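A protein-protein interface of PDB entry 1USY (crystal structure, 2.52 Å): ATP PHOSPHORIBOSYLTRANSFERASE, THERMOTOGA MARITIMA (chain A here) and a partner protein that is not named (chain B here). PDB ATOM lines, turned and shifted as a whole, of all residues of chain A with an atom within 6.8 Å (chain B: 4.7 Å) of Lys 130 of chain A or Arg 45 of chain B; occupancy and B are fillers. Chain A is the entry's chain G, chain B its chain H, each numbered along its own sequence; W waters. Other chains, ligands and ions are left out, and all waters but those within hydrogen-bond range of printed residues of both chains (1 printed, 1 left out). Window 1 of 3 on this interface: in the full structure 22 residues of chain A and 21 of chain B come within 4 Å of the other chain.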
ATOM      1  N   ARG A  45     -18.276  13.060   4.986  1.00  0.00           N
ATOM      2  CA  ARG A  45     -18.411  13.797   6.245  1.00  0.00           C
ATOM      3  C   ARG A  45     -19.006  15.191   6.082  1.00  0.00           C
ATOM      4  O   ARG A  45     -18.696  15.883   5.115  1.00  0.00           O
ATOM      5  CB  ARG A  45     -17.057  13.910   6.934  1.00  0.00           C
ATOM      6  CG  ARG A  45     -16.562  12.570   7.388  1.00  0.00           C
ATOM      7  CD  ARG A  45     -17.011  12.255   8.788  1.00  0.00           C
ATOM      8  NE  ARG A  45     -16.887  10.834   9.075  1.00  0.00           N
ATOM      9  CZ  ARG A  45     -17.846  10.113   9.642  1.00  0.00           C
ATOM     10  NH1 ARG A  45     -18.998  10.688   9.993  1.00  0.00           N
ATOM     11  NH2 ARG A  45     -17.648   8.819   9.875  1.00  0.00           N
ATOM     12  N   THR A 107     -12.115  23.378  20.342  1.00  0.00           N
ATOM     13  CA  THR A 107     -13.251  23.365  19.376  1.00  0.00           C
ATOM     14  C   THR A 107     -13.041  22.506  18.112  1.00  0.00           C
ATOM     15  O   THR A 107     -11.922  22.233  17.710  1.00  0.00           O
ATOM     16  CB  THR A 107     -13.638  24.841  18.983  1.00  0.00           C
ATOM     17  OG1 THR A 107     -14.596  24.871  17.914  1.00  0.00           O
ATOM     18  CG2 THR A 107     -12.449  25.569  18.402  1.00  0.00           C
ATOM     19  N   LYS A 108     -14.130  22.082  17.494  1.00  0.00           N
ATOM     20  CA  LYS A 108     -14.052  21.487  16.168  1.00  0.00           C
ATOM     21  C   LYS A 108     -14.099  22.580  15.126  1.00  0.00           C
ATOM     22  O   LYS A 108     -13.968  22.283  13.924  1.00  0.00           O
ATOM     23  CB  LYS A 108     -15.287  20.656  15.840  1.00  0.00           C
ATOM     24  CG  LYS A 108     -15.579  19.462  16.678  1.00  0.00           C
ATOM     25  CD  LYS A 108     -16.719  18.697  16.053  1.00  0.00           C
ATOM     26  CE  LYS A 108     -17.379  17.854  17.110  1.00  0.00           C
ATOM     27  NZ  LYS A 108     -18.837  17.672  16.826  1.00  0.00           N
ATOM     28  N   PRO A 128      -7.548  22.908  18.372  1.00  0.00           N
ATOM     29  CA  PRO A 128      -8.497  22.146  17.549  1.00  0.00           C
ATOM     30  C   PRO A 128      -8.610  20.715  18.057  1.00  0.00           C
ATOM     31  O   PRO A 128      -7.616  20.118  18.486  1.00  0.00           O
ATOM     32  CB  PRO A 128      -7.880  22.174  16.127  1.00  0.00           C
ATOM     33  CG  PRO A 128      -6.472  22.784  16.261  1.00  0.00           C
ATOM     34  CD  PRO A 128      -6.253  23.152  17.702  1.00  0.00           C
ATOM     35  N   LEU A 129      -9.831  20.204  18.043  1.00  0.00           N
ATOM     36  CA  LEU A 129     -10.126  18.835  18.457  1.00  0.00           C
ATOM     37  C   LEU A 129     -11.135  18.304  17.481  1.00  0.00           C
ATOM     38  O   LEU A 129     -11.759  19.048  16.726  1.00  0.00           O
ATOM     39  CB  LEU A 129     -10.708  18.794  19.859  1.00  0.00           C
ATOM     40  CG  LEU A 129      -9.716  19.148  20.970  1.00  0.00           C
ATOM     41  CD1 LEU A 129     -10.423  19.315  22.357  1.00  0.00           C
ATOM     42  CD2 LEU A 129      -8.567  18.157  21.021  1.00  0.00           C
ATOM     43  N   LYS A 130     -11.277  17.003  17.460  1.00  0.00           N
ATOM     44  CA  LYS A 130     -12.064  16.400  16.428  1.00  0.00           C
ATOM     45  C   LYS A 130     -13.389  15.934  17.039  1.00  0.00           C
ATOM     46  O   LYS A 130     -14.267  15.443  16.352  1.00  0.00           O
ATOM     47  CB  LYS A 130     -11.229  15.302  15.770  1.00  0.00           C
ATOM     48  CG  LYS A 130     -10.112  15.901  14.889  1.00  0.00           C
ATOM     49  CD  LYS A 130      -9.493  14.911  13.853  1.00  0.00           C
ATOM     50  CE  LYS A 130     -10.483  14.421  12.825  1.00  0.00           C
ATOM     51  NZ  LYS A 130     -11.731  13.960  13.532  1.00  0.00           N
ATOM     52  N   GLY A 131     -13.532  16.146  18.344  1.00  0.00           N
ATOM     53  CA  GLY A 131     -14.682  15.670  19.059  1.00  0.00           C
ATOM     54  C   GLY A 131     -14.378  15.645  20.524  1.00  0.00           C
ATOM     55  O   GLY A 131     -13.300  16.063  20.916  1.00  0.00           O
ATOM     56  N   SER A 132     -15.339  15.157  21.311  1.00  0.00           N
ATOM     57  CA  SER A 132     -15.262  15.058  22.790  1.00  0.00           C
ATOM     58  C   SER A 132     -14.840  16.376  23.450  1.00  0.00           C
ATOM     59  O   SER A 132     -14.314  16.417  24.563  1.00  0.00           O
ATOM     60  CB  SER A 132     -14.382  13.878  23.232  1.00  0.00           C
ATOM     61  OG  SER A 132     -14.701  12.712  22.501  1.00  0.00           O
ATOM     62  N   VAL A 133     -15.131  17.441  22.741  1.00  0.00           N
ATOM     63  CA  VAL A 133     -14.773  18.788  23.088  1.00  0.00           C
ATOM     64  C   VAL A 133     -15.101  19.240  24.507  1.00  0.00           C
ATOM     65  O   VAL A 133     -14.463  20.150  24.986  1.00  0.00           O
ATOM     66  CB  VAL A 133     -15.447  19.696  22.089  1.00  0.00           C
ATOM     67  CG1 VAL A 133     -15.183  21.166  22.366  1.00  0.00           C
ATOM     68  CG2 VAL A 133     -14.985  19.324  20.689  1.00  0.00           C
ATOM     69  N   LYS B   8     -11.542   6.823  20.965  1.00  0.00           N
ATOM     70  CA  LYS B   8     -12.915   6.421  20.636  1.00  0.00           C
ATOM     71  C   LYS B   8     -13.007   5.662  19.300  1.00  0.00           C
ATOM     72  O   LYS B   8     -12.288   5.968  18.357  1.00  0.00           O
ATOM     73  CB  LYS B   8     -13.823   7.664  20.593  1.00  0.00           C
ATOM     74  CG  LYS B   8     -14.457   8.018  21.932  1.00  0.00           C
ATOM     75  CD  LYS B   8     -15.517   9.051  21.766  1.00  0.00           C
ATOM     76  CE  LYS B   8     -16.650   8.773  22.711  1.00  0.00           C
ATOM     77  NZ  LYS B   8     -17.727   9.797  22.566  1.00  0.00           N
ATOM     78  N   MET B  43     -12.231   9.871  27.047  1.00  0.00           N
ATOM     79  CA  MET B  43     -12.670   9.189  25.848  1.00  0.00           C
ATOM     80  C   MET B  43     -12.671  10.251  24.764  1.00  0.00           C
ATOM     81  O   MET B  43     -13.598  11.028  24.613  1.00  0.00           O
ATOM     82  CB  MET B  43     -14.068   8.551  26.038  1.00  0.00           C
ATOM     83  CG  MET B  43     -14.249   7.681  27.335  1.00  0.00           C
ATOM     84  SD  MET B  43     -13.037   6.336  27.544  1.00  0.00           S
ATOM     85  CE  MET B  43     -13.351   5.477  26.006  1.00  0.00           C
ATOM     86  N   VAL B  44     -11.604  10.252  23.997  1.00  0.00           N
ATOM     87  CA  VAL B  44     -11.286  11.329  23.109  1.00  0.00           C
ATOM     88  C   VAL B  44     -11.078  10.739  21.708  1.00  0.00           C
ATOM     89  O   VAL B  44     -11.107   9.530  21.539  1.00  0.00           O
ATOM     90  CB  VAL B  44     -10.020  12.025  23.636  1.00  0.00           C
ATOM     91  CG1 VAL B  44      -8.790  11.266  23.193  1.00  0.00           C
ATOM     92  CG2 VAL B  44      -9.952  13.435  23.151  1.00  0.00           C
ATOM     93  N   ARG B  45     -10.905  11.571  20.698  1.00  0.00           N
ATOM     94  CA  ARG B  45     -10.779  11.047  19.358  1.00  0.00           C
ATOM     95  C   ARG B  45      -9.338  10.676  19.101  1.00  0.00           C
ATOM     96  O   ARG B  45      -8.436  11.278  19.682  1.00  0.00           O
ATOM     97  CB  ARG B  45     -11.265  12.056  18.339  1.00  0.00           C
ATOM     98  CG  ARG B  45     -12.723  12.280  18.408  1.00  0.00           C
ATOM     99  CD  ARG B  45     -13.470  11.824  17.195  1.00  0.00           C
ATOM    100  NE  ARG B  45     -14.825  12.371  17.161  1.00  0.00           N
ATOM    101  CZ  ARG B  45     -15.486  12.727  16.050  1.00  0.00           C
ATOM    102  NH1 ARG B  45     -14.917  12.616  14.843  1.00  0.00           N
ATOM    103  NH2 ARG B  45     -16.735  13.202  16.150  1.00  0.00           N
ATOM    104  N   PRO B  46      -9.115   9.707  18.216  1.00  0.00           N
ATOM    105  CA  PRO B  46      -7.805   9.090  18.091  1.00  0.00           C
ATOM    106  C   PRO B  46      -6.761  10.113  17.709  1.00  0.00           C
ATOM    107  O   PRO B  46      -5.683  10.079  18.328  1.00  0.00           O
ATOM    108  CB  PRO B  46      -8.004   8.001  17.024  1.00  0.00           C
ATOM    109  CG  PRO B  46      -9.212   8.360  16.325  1.00  0.00           C
ATOM    110  CD  PRO B  46     -10.080   9.134  17.271  1.00  0.00           C
ATOM    111  N   PHE B  47      -7.079  11.031  16.796  1.00  0.00           N
ATOM    112  CA  PHE B  47      -6.162  12.097  16.431  1.00  0.00           C
ATOM    113  C   PHE B  47      -5.813  12.986  17.615  1.00  0.00           C
ATOM    114  O   PHE B  47      -4.741  13.612  17.646  1.00  0.00           O
ATOM    115  CB  PHE B  47      -6.790  13.002  15.391  1.00  0.00           C
ATOM    116  CG  PHE B  47      -6.372  12.748  13.967  1.00  0.00           C
ATOM    117  CD1 PHE B  47      -5.770  13.773  13.228  1.00  0.00           C
ATOM    118  CD2 PHE B  47      -6.715  11.559  13.310  1.00  0.00           C
ATOM    119  CE1 PHE B  47      -5.441  13.587  11.867  1.00  0.00           C
ATOM    120  CE2 PHE B  47      -6.401  11.363  11.956  1.00  0.00           C
ATOM    121  CZ  PHE B  47      -5.762  12.374  11.234  1.00  0.00           C
ATOM    122  N   ASP B  48      -6.710  13.078  18.582  1.00  0.00           N
ATOM    123  CA  ASP B  48      -6.461  13.943  19.729  1.00  0.00           C
ATOM    124  C   ASP B  48      -5.665  13.370  20.902  1.00  0.00           C
ATOM    125  O   ASP B  48      -5.379  14.088  21.847  1.00  0.00           O
ATOM    126  CB  ASP B  48      -7.769  14.553  20.209  1.00  0.00           C
ATOM    127  CG  ASP B  48      -8.361  15.493  19.175  1.00  0.00           C
ATOM    128  OD1 ASP B  48      -7.535  16.193  18.534  1.00  0.00           O
ATOM    129  OD2 ASP B  48      -9.603  15.615  18.957  1.00  0.00           O
ATOM    130  N   VAL B  49      -5.271  12.107  20.820  1.00  0.00           N
ATOM    131  CA  VAL B  49      -4.519  11.483  21.896  1.00  0.00           C
ATOM    132  C   VAL B  49      -3.222  12.210  22.165  1.00  0.00           C
ATOM    133  O   VAL B  49      -2.968  12.605  23.305  1.00  0.00           O
ATOM    134  CB  VAL B  49      -4.225  10.010  21.622  1.00  0.00           C
ATOM    135  CG1 VAL B  49      -2.935   9.598  22.337  1.00  0.00           C
ATOM    136  CG2 VAL B  49      -5.395   9.165  22.054  1.00  0.00           C
HETATM  137  O   HOH W   1     -12.356  11.566  14.393  1.00  0.00           O
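Among the printed residues, pairs that only touch across the chains: Leu 129 of chain A with Asp 48 of chain B, Lys 130 of chain A with Phe 47 of chain B, Ser 132 of chain A with Val 44 of chain B, Gly 131 of chain A with Arg 45 of chain B, Ser 132 of chain A with Lys 8 of chain B and Pro 128 of chain A with Asp 48 of chain B.
The guanidinium group of Arg 45 of chain B lies close to the backbone carbonyl oxygen of Lys 130 of chain A (3.2 Å). N of Lys 130 of chain A sits at hydrogen-bond distance from OD2 of Asp 48 of chain B (2.6 Å). The side-chain hydroxyl (OG) of Ser 132 of chain A lies within hydrogen-bond range of the backbone carbonyl oxygen (O) of Met 43 of chain B.
Printed residues of chain B that touch a printed residue of chain A: Lys 8, Met 43, Val 44, Arg 45, Phe 47 and Asp 48. Hydrophobic or aromatic side chains of chain A that line the printed part of chain B: Leu 129. Among the printed residues, 9 pairs touch across the chains. Among the printed residues, no Asp or Glu carboxylate lies within 4 Å of a Lys or Arg side-chain nitrogen of the other chain.
The backbone carbonyl oxygen (O) of Thr 107 of chain A sits at hydrogen-bond distance from the backbone NH (N) of Leu 129 of chain A (2.9 Å). The backbone NH (N) of Lys 8 of chain B lies within hydrogen-bond range of the backbone carbonyl oxygen (O) of Val 44 of chain B (2.8 Å).
Arg 45 of chain B touches two residues of chain A. Of the printed residues of chain A, Met 43 of chain B touches Ser 132 (2.9 Å). Printed residues of chain A within 4 Å of Phe 47 of chain B: Lys 130 (3.6 Å). Printed residues of chain B within 4 Å of Leu 129 of chain A: Asp 48. Printed residues of chain B within 4 Å of Gly 131 of chain A: Arg 45. Printed residues of chain B within 4 Å of Pro 128 of chain A: Asp 48 (3.9 Å). Arg 45 of chain A touches none of the printed residues of chain B. The nearest printed residue of chain B that does not touch Lys 130 of chain A is Pro 46 of chain B (6.3 Å). The nearest printed residue of chain B that does not touch Ser 132 of chain A is Arg 45 of chain B (4.4 Å).
Water W1 lies within hydrogen-bond range of the side-chain amino group (NZ) of Lys 130 of chain A (2.6 Å) and the guanidinium group (NH1) of Arg 45 of chain B (2.8 Å).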
